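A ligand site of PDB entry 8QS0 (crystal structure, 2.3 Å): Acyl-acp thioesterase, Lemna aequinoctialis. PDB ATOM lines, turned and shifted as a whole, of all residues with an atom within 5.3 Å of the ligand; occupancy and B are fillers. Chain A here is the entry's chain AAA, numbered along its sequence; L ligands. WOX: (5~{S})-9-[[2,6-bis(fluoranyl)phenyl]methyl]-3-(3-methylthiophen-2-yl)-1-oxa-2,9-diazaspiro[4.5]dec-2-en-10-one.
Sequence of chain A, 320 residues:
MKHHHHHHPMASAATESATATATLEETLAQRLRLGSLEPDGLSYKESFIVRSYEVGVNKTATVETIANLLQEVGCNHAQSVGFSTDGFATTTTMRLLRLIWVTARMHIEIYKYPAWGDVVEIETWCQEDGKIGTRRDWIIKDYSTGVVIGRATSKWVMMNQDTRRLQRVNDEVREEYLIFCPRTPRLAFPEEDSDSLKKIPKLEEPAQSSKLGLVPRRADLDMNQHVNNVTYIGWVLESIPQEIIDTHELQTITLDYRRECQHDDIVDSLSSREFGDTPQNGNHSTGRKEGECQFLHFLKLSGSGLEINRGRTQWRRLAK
O9 of the ligand lies close to SG of Cys 126 (3.8 Å).
The guanidinium group (NH2) of Arg 136 is in hydrogen-bond range of an oxygen (O25) of the ligand (2.7 Å).
O of Gln 71 lies within hydrogen-bond range of SG of Cys 75 (3.4 Å).
NH2 of Arg 136 lies within hydrogen-bond range of SG of Cys 126, at 3.2 Å.
The backbone carbonyl oxygen (O) of Arg 136 sits at hydrogen-bond distance from the backbone NH (N) of Ser 154, 2.8 Å away.
The backbone carbonyl oxygen of Tyr 177 lies within hydrogen-bond range of the side-chain sulfur of Cys 181, at 3.5 Å.
The backbone carbonyl oxygen of Arg 135 lies close to the side-chain sulfur of Cys 126, at 3.8 Å.
The backbone carbonyl oxygen (O) of Thr 134 is in hydrogen-bond range of the backbone NH (N) of Trp 156 (2.8 Å).
The guanidinium group (NH1) of Arg 136 is in hydrogen-bond range of a ring nitrogen (ND1) of His 77 (2.9 Å).
O of Ala 78 is in hydrogen-bond range of N of Phe 83, 3.1 Å away.
Merely in contact with the ligand: Thr 134, Ala 78, Tyr 177, Phe 83, Trp 156, Trp 101, Phe 180, His 77, Cys 181, Val 81, Gln 71, Ala 89 and Gly 74.
Hydrophobic or aromatic side chains within 4 Å of the ligand: His 77, Ala 78, Val 81, Phe 83, Ala 89, Trp 101, Trp 156, Tyr 177 and Phe 180.
15 residues have an atom within 4 Å of the ligand: Gln 71, Gly 74, His 77, Ala 78, Val 81, Phe 83, Ala 89, Trp 101, Cys 126, Thr 134, Arg 136, Trp 156, Tyr 177, Phe 180 and Cys 181.
Along chain A the residues within 4 Å of the ligand span positions 71 to 181.
The nearest printed residue that does not touch the ligand is Trp 138 (4.05 Å).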
ATOM      1  N   LEU A  70      -5.019  16.504   5.504  1.00  0.00           N
ATOM      2  CA  LEU A  70      -3.985  16.595   6.576  1.00  0.00           C
ATOM      3  C   LEU A  70      -2.607  16.628   5.922  1.00  0.00           C
ATOM      4  O   LEU A  70      -1.783  17.487   6.291  1.00  0.00           O
ATOM      5  CB  LEU A  70      -4.056  15.389   7.517  1.00  0.00           C
ATOM      6  CG  LEU A  70      -5.346  15.229   8.319  1.00  0.00           C
ATOM      7  CD1 LEU A  70      -5.278  13.958   9.127  1.00  0.00           C
ATOM      8  CD2 LEU A  70      -5.562  16.429   9.227  1.00  0.00           C
ATOM      9  N   GLN A  71      -2.358  15.707   4.981  1.00  0.00           N
ATOM     10  CA  GLN A  71      -1.091  15.672   4.221  1.00  0.00           C
ATOM     11  C   GLN A  71      -0.902  16.993   3.467  1.00  0.00           C
ATOM     12  O   GLN A  71       0.209  17.553   3.520  1.00  0.00           O
ATOM     13  CB  GLN A  71      -1.074  14.512   3.228  1.00  0.00           C
ATOM     14  CG  GLN A  71      -0.230  14.807   1.999  1.00  0.00           C
ATOM     15  CD  GLN A  71       0.459  13.566   1.478  1.00  0.00           C
ATOM     16  OE1 GLN A  71       1.680  13.461   1.534  1.00  0.00           O
ATOM     17  NE2 GLN A  71      -0.339  12.633   0.981  1.00  0.00           N
ATOM     18  N   GLY A  74       0.220  19.810   5.703  1.00  0.00           N
ATOM     19  CA  GLY A  74       1.606  19.463   6.084  1.00  0.00           C
ATOM     20  C   GLY A  74       2.607  19.913   5.037  1.00  0.00           C
ATOM     21  O   GLY A  74       3.550  20.647   5.377  1.00  0.00           O
ATOM     22  N   CYS A  75       2.399  19.504   3.776  1.00  0.00           N
ATOM     23  CA  CYS A  75       3.282  19.829   2.618  1.00  0.00           C
ATOM     24  C   CYS A  75       3.345  21.353   2.436  1.00  0.00           C
ATOM     25  O   CYS A  75       4.469  21.864   2.259  1.00  0.00           O
ATOM     26  CB  CYS A  75       2.815  19.157   1.346  1.00  0.00           C
ATOM     27  SG  CYS A  75       2.939  17.351   1.424  1.00  0.00           S
ATOM     28  N   HIS A  77       2.784  23.745   4.652  1.00  0.00           N
ATOM     29  CA  HIS A  77       3.544  24.204   5.856  1.00  0.00           C
ATOM     30  C   HIS A  77       5.039  24.006   5.616  1.00  0.00           C
ATOM     31  O   HIS A  77       5.821  24.947   5.867  1.00  0.00           O
ATOM     32  CB  HIS A  77       3.128  23.420   7.102  1.00  0.00           C
ATOM     33  CG  HIS A  77       3.706  23.944   8.365  1.00  0.00           C
ATOM     34  ND1 HIS A  77       3.603  23.281   9.554  1.00  0.00           N
ATOM     35  CD2 HIS A  77       4.394  25.089   8.621  1.00  0.00           C
ATOM     36  CE1 HIS A  77       4.182  23.997  10.503  1.00  0.00           C
ATOM     37  NE2 HIS A  77       4.671  25.110   9.956  1.00  0.00           N
ATOM     38  N   ALA A  78       5.422  22.820   5.186  1.00  0.00           N
ATOM     39  CA  ALA A  78       6.837  22.481   4.942  1.00  0.00           C
ATOM     40  C   ALA A  78       7.397  23.488   3.924  1.00  0.00           C
ATOM     41  O   ALA A  78       8.426  24.122   4.233  1.00  0.00           O
ATOM     42  CB  ALA A  78       6.986  21.044   4.505  1.00  0.00           C
ATOM     43  N   VAL A  81       8.101  27.270   5.189  1.00  0.00           N
ATOM     44  CA  VAL A  81       9.289  27.522   6.059  1.00  0.00           C
ATOM     45  C   VAL A  81      10.554  26.890   5.450  1.00  0.00           C
ATOM     46  O   VAL A  81      11.564  26.808   6.164  1.00  0.00           O
ATOM     47  CB  VAL A  81       9.071  27.079   7.515  1.00  0.00           C
ATOM     48  CG1 VAL A  81       7.846  27.752   8.103  1.00  0.00           C
ATOM     49  CG2 VAL A  81       9.000  25.567   7.662  1.00  0.00           C
ATOM     50  N   PHE A  83      11.509  23.890   3.854  1.00  0.00           N
ATOM     51  CA  PHE A  83      11.907  22.453   3.797  1.00  0.00           C
ATOM     52  C   PHE A  83      11.600  21.919   2.403  1.00  0.00           C
ATOM     53  O   PHE A  83      11.120  22.726   1.573  1.00  0.00           O
ATOM     54  CB  PHE A  83      11.268  21.664   4.945  1.00  0.00           C
ATOM     55  CG  PHE A  83      11.729  22.095   6.321  1.00  0.00           C
ATOM     56  CD1 PHE A  83      12.988  22.644   6.510  1.00  0.00           C
ATOM     57  CD2 PHE A  83      10.905  21.941   7.420  1.00  0.00           C
ATOM     58  CE1 PHE A  83      13.410  23.043   7.768  1.00  0.00           C
ATOM     59  CE2 PHE A  83      11.335  22.339   8.685  1.00  0.00           C
ATOM     60  CZ  PHE A  83      12.588  22.868   8.860  1.00  0.00           C
ATOM     61  N   GLY A  87       8.847  16.403  -1.163  1.00  0.00           N
ATOM     62  CA  GLY A  87       8.215  15.130  -0.768  1.00  0.00           C
ATOM     63  C   GLY A  87       8.650  14.633   0.613  1.00  0.00           C
ATOM     64  O   GLY A  87       7.834  13.875   1.210  1.00  0.00           O
ATOM     65  N   PHE A  88       9.861  14.975   1.103  1.00  0.00           N
ATOM     66  CA  PHE A  88      10.473  14.321   2.299  1.00  0.00           C
ATOM     67  C   PHE A  88      10.708  15.280   3.478  1.00  0.00           C
ATOM     68  O   PHE A  88      11.216  14.799   4.512  1.00  0.00           O
ATOM     69  CB  PHE A  88      11.754  13.563   1.907  1.00  0.00           C
ATOM     70  CG  PHE A  88      11.518  12.141   1.411  1.00  0.00           C
ATOM     71  CD1 PHE A  88      11.278  11.110   2.312  1.00  0.00           C
ATOM     72  CD2 PHE A  88      11.513  11.846   0.064  1.00  0.00           C
ATOM     73  CE1 PHE A  88      11.049   9.818   1.870  1.00  0.00           C
ATOM     74  CE2 PHE A  88      11.296  10.545  -0.377  1.00  0.00           C
ATOM     75  CZ  PHE A  88      11.070   9.534   0.527  1.00  0.00           C
ATOM     76  N   ALA A  89      10.336  16.556   3.341  1.00  0.00           N
ATOM     77  CA  ALA A  89      10.451  17.601   4.399  1.00  0.00           C
ATOM     78  C   ALA A  89      11.847  17.581   5.053  1.00  0.00           C
ATOM     79  O   ALA A  89      11.926  17.584   6.302  1.00  0.00           O
ATOM     80  CB  ALA A  89       9.368  17.405   5.434  1.00  0.00           C
ATOM     81  N   TRP A 101      12.645  11.841   6.773  1.00  0.00           N
ATOM     82  CA  TRP A 101      11.565  11.592   7.773  1.00  0.00           C
ATOM     83  C   TRP A 101      10.790  10.349   7.330  1.00  0.00           C
ATOM     84  O   TRP A 101      10.503  10.225   6.153  1.00  0.00           O
ATOM     85  CB  TRP A 101      10.634  12.803   7.901  1.00  0.00           C
ATOM     86  CG  TRP A 101      11.291  13.989   8.531  1.00  0.00           C
ATOM     87  CD1 TRP A 101      11.636  15.170   7.918  1.00  0.00           C
ATOM     88  CD2 TRP A 101      11.746  14.095   9.881  1.00  0.00           C
ATOM     89  NE1 TRP A 101      12.248  16.009   8.813  1.00  0.00           N
ATOM     90  CE2 TRP A 101      12.329  15.379  10.029  1.00  0.00           C
ATOM     91  CE3 TRP A 101      11.693  13.248  10.998  1.00  0.00           C
ATOM     92  CZ2 TRP A 101      12.863  15.820  11.245  1.00  0.00           C
ATOM     93  CZ3 TRP A 101      12.225  13.685  12.184  1.00  0.00           C
ATOM     94  CH2 TRP A 101      12.815  14.943  12.301  1.00  0.00           C
ATOM     95  N   CYS A 126       4.399  21.379  14.206  1.00  0.00           N
ATOM     96  CA  CYS A 126       5.308  20.258  14.581  1.00  0.00           C
ATOM     97  C   CYS A 126       5.843  20.506  15.981  1.00  0.00           C
ATOM     98  O   CYS A 126       5.782  21.664  16.463  1.00  0.00           O
ATOM     99  CB  CYS A 126       6.429  20.104  13.556  1.00  0.00           C
ATOM    100  SG  CYS A 126       5.841  19.496  11.958  1.00  0.00           S
ATOM    101  N   THR A 134       9.873  13.339  15.994  1.00  0.00           N
ATOM    102  CA  THR A 134       9.148  14.616  15.833  1.00  0.00           C
ATOM    103  C   THR A 134       7.658  14.302  15.645  1.00  0.00           C
ATOM    104  O   THR A 134       7.354  13.256  15.057  1.00  0.00           O
ATOM    105  CB  THR A 134       9.729  15.434  14.683  1.00  0.00           C
ATOM    106  OG1 THR A 134       9.567  14.653  13.494  1.00  0.00           O
ATOM    107  CG2 THR A 134      11.177  15.777  14.911  1.00  0.00           C
ATOM    108  N   ARG A 135       6.797  15.161  16.164  1.00  0.00           N
ATOM    109  CA  ARG A 135       5.331  15.102  15.980  1.00  0.00           C
ATOM    110  C   ARG A 135       4.923  16.139  14.935  1.00  0.00           C
ATOM    111  O   ARG A 135       5.527  17.234  14.950  1.00  0.00           O
ATOM    112  CB  ARG A 135       4.587  15.389  17.282  1.00  0.00           C
ATOM    113  CG  ARG A 135       4.395  14.162  18.156  1.00  0.00           C
ATOM    114  CD  ARG A 135       3.800  14.438  19.530  1.00  0.00           C
ATOM    115  NE  ARG A 135       2.995  15.660  19.496  1.00  0.00           N
ATOM    116  CZ  ARG A 135       3.249  16.782  20.162  1.00  0.00           C
ATOM    117  NH1 ARG A 135       4.300  16.850  20.960  1.00  0.00           N
ATOM    118  NH2 ARG A 135       2.453  17.826  20.042  1.00  0.00           N
ATOM    119  N   ARG A 136       3.962  15.787  14.071  1.00  0.00           N
ATOM    120  CA  ARG A 136       3.017  16.747  13.450  1.00  0.00           C
ATOM    121  C   ARG A 136       1.622  16.523  14.032  1.00  0.00           C
ATOM    122  O   ARG A 136       1.169  15.381  14.014  1.00  0.00           O
ATOM    123  CB  ARG A 136       2.945  16.592  11.935  1.00  0.00           C
ATOM    124  CG  ARG A 136       2.104  17.665  11.283  1.00  0.00           C
ATOM    125  CD  ARG A 136       2.250  17.706   9.780  1.00  0.00           C
ATOM    126  NE  ARG A 136       3.488  18.386   9.385  1.00  0.00           N
ATOM    127  CZ  ARG A 136       3.672  19.700   9.417  1.00  0.00           C
ATOM    128  NH1 ARG A 136       2.714  20.511   9.834  1.00  0.00           N
ATOM    129  NH2 ARG A 136       4.820  20.213   9.008  1.00  0.00           N
ATOM    130  N   TRP A 138      -2.565  18.121  13.966  1.00  0.00           N
ATOM    131  CA  TRP A 138      -3.559  18.907  13.218  1.00  0.00           C
ATOM    132  C   TRP A 138      -4.805  19.113  14.090  1.00  0.00           C
ATOM    133  O   TRP A 138      -5.167  18.186  14.831  1.00  0.00           O
ATOM    134  CB  TRP A 138      -3.951  18.170  11.935  1.00  0.00           C
ATOM    135  CG  TRP A 138      -2.891  17.841  10.940  1.00  0.00           C
ATOM    136  CD1 TRP A 138      -2.682  18.470   9.757  1.00  0.00           C
ATOM    137  CD2 TRP A 138      -2.024  16.688  10.934  1.00  0.00           C
ATOM    138  NE1 TRP A 138      -1.697  17.840   9.039  1.00  0.00           N
ATOM    139  CE2 TRP A 138      -1.270  16.746   9.737  1.00  0.00           C
ATOM    140  CE3 TRP A 138      -1.757  15.648  11.831  1.00  0.00           C
ATOM    141  CZ2 TRP A 138      -0.315  15.783   9.409  1.00  0.00           C
ATOM    142  CZ3 TRP A 138      -0.824  14.702  11.502  1.00  0.00           C
ATOM    143  CH2 TRP A 138      -0.102  14.777  10.315  1.00  0.00           C
ATOM    144  N   SER A 154       0.808  12.625  14.523  1.00  0.00           N
ATOM    145  CA  SER A 154       1.713  11.689  13.808  1.00  0.00           C
ATOM    146  C   SER A 154       3.106  11.759  14.423  1.00  0.00           C
ATOM    147  O   SER A 154       3.549  12.876  14.804  1.00  0.00           O
ATOM    148  CB  SER A 154       1.739  12.019  12.345  1.00  0.00           C
ATOM    149  OG  SER A 154       2.143  13.372  12.174  1.00  0.00           O
ATOM    150  N   TRP A 156       7.112  10.800  13.689  1.00  0.00           N
ATOM    151  CA  TRP A 156       8.100  10.691  12.597  1.00  0.00           C
ATOM    152  C   TRP A 156       9.455  10.405  13.232  1.00  0.00           C
ATOM    153  O   TRP A 156       9.718  10.942  14.319  1.00  0.00           O
ATOM    154  CB  TRP A 156       8.105  11.977  11.769  1.00  0.00           C
ATOM    155  CG  TRP A 156       6.781  12.328  11.161  1.00  0.00           C
ATOM    156  CD1 TRP A 156       5.717  12.921  11.774  1.00  0.00           C
ATOM    157  CD2 TRP A 156       6.390  12.130   9.791  1.00  0.00           C
ATOM    158  NE1 TRP A 156       4.689  13.080  10.896  1.00  0.00           N
ATOM    159  CE2 TRP A 156       5.068  12.605   9.680  1.00  0.00           C
ATOM    160  CE3 TRP A 156       7.034  11.599   8.671  1.00  0.00           C
ATOM    161  CZ2 TRP A 156       4.378  12.568   8.466  1.00  0.00           C
ATOM    162  CZ3 TRP A 156       6.348  11.545   7.480  1.00  0.00           C
ATOM    163  CH2 TRP A 156       5.043  12.030   7.382  1.00  0.00           C
ATOM    164  N   TYR A 177      15.001  22.448  12.529  1.00  0.00           N
ATOM    165  CA  TYR A 177      13.504  22.397  12.429  1.00  0.00           C
ATOM    166  C   TYR A 177      12.867  22.931  13.714  1.00  0.00           C
ATOM    167  O   TYR A 177      11.719  23.391  13.612  1.00  0.00           O
ATOM    168  CB  TYR A 177      12.993  21.012  12.015  1.00  0.00           C
ATOM    169  CG  TYR A 177      13.194  19.923  13.041  1.00  0.00           C
ATOM    170  CD1 TYR A 177      12.364  19.797  14.154  1.00  0.00           C
ATOM    171  CD2 TYR A 177      14.215  19.018  12.900  1.00  0.00           C
ATOM    172  CE1 TYR A 177      12.564  18.811  15.096  1.00  0.00           C
ATOM    173  CE2 TYR A 177      14.426  18.010  13.823  1.00  0.00           C
ATOM    174  CZ  TYR A 177      13.611  17.926  14.930  1.00  0.00           C
ATOM    175  OH  TYR A 177      13.836  16.926  15.838  1.00  0.00           O
ATOM    176  N   PHE A 180      11.107  26.363  14.003  1.00  0.00           N
ATOM    177  CA  PHE A 180       9.781  26.546  13.355  1.00  0.00           C
ATOM    178  C   PHE A 180       8.690  25.780  14.117  1.00  0.00           C
ATOM    179  O   PHE A 180       7.645  25.538  13.519  1.00  0.00           O
ATOM    180  CB  PHE A 180       9.816  26.065  11.900  1.00  0.00           C
ATOM    181  CG  PHE A 180      10.865  26.725  11.037  1.00  0.00           C
ATOM    182  CD1 PHE A 180      10.757  28.052  10.679  1.00  0.00           C
ATOM    183  CD2 PHE A 180      11.937  25.995  10.551  1.00  0.00           C
ATOM    184  CE1 PHE A 180      11.706  28.639   9.868  1.00  0.00           C
ATOM    185  CE2 PHE A 180      12.894  26.581   9.746  1.00  0.00           C
ATOM    186  CZ  PHE A 180      12.780  27.913   9.412  1.00  0.00           C
ATOM    187  N   CYS A 181       8.954  25.452  15.381  1.00  0.00           N
ATOM    188  CA  CYS A 181       8.008  24.731  16.296  1.00  0.00           C
ATOM    189  C   CYS A 181       7.716  25.614  17.497  1.00  0.00           C
ATOM    190  O   CYS A 181       8.580  26.352  17.946  1.00  0.00           O
ATOM    191  CB  CYS A 181       8.585  23.408  16.775  1.00  0.00           C
ATOM    192  SG  CYS A 181       8.920  22.259  15.412  1.00  0.00           S
HETATM  193  C1  WOX L   1       2.614  15.670   6.618  1.00  0.00           C
HETATM  194  C2  WOX L   1       3.826  15.244   5.826  1.00  0.00           C
HETATM  195  C3  WOX L   1       3.712  14.806   4.524  1.00  0.00           C
HETATM  196  C4  WOX L   1       4.874  14.450   3.932  1.00  0.00           C
HETATM  197  C6  WOX L   1       5.113  15.251   6.285  1.00  0.00           C
HETATM  198  C11 WOX L   1       8.014  15.665  10.306  1.00  0.00           C
HETATM  199  C17 WOX L   1       9.013  21.133  11.171  1.00  0.00           C
HETATM  200  S5  WOX L   1       6.252  14.691   5.030  1.00  0.00           S
HETATM  201  C7  WOX L   1       5.576  15.660   7.607  1.00  0.00           C
HETATM  202  N8  WOX L   1       4.899  16.086   8.614  1.00  0.00           N
HETATM  203  O9  WOX L   1       5.706  16.394   9.773  1.00  0.00           O
HETATM  204  C10 WOX L   1       7.078  16.439   9.346  1.00  0.00           C
HETATM  205  C12 WOX L   1       8.782  16.620  11.233  1.00  0.00           C
HETATM  206  C13 WOX L   1       9.609  17.537  10.350  1.00  0.00           C
HETATM  207  N14 WOX L   1       8.730  18.307   9.494  1.00  0.00           N
HETATM  208  C15 WOX L   1       9.229  19.651   9.116  1.00  0.00           C
HETATM  209  C16 WOX L   1       8.668  20.846   9.850  1.00  0.00           C
HETATM  210  F18 WOX L   1       9.861  20.318  11.879  1.00  0.00           F
HETATM  211  C19 WOX L   1       8.482  22.280  11.781  1.00  0.00           C
HETATM  212  C20 WOX L   1       7.640  23.138  11.060  1.00  0.00           C
HETATM  213  C21 WOX L   1       7.338  22.861   9.738  1.00  0.00           C
HETATM  214  C22 WOX L   1       7.873  21.719   9.141  1.00  0.00           C
HETATM  215  F23 WOX L   1       7.566  21.424   7.852  1.00  0.00           F
HETATM  216  C24 WOX L   1       7.566  17.841   9.043  1.00  0.00           C
HETATM  217  O25 WOX L   1       6.904  18.585   8.317  1.00  0.00           O
HETATM  218  C26 WOX L   1       7.020  15.593   8.050  1.00  0.00           C
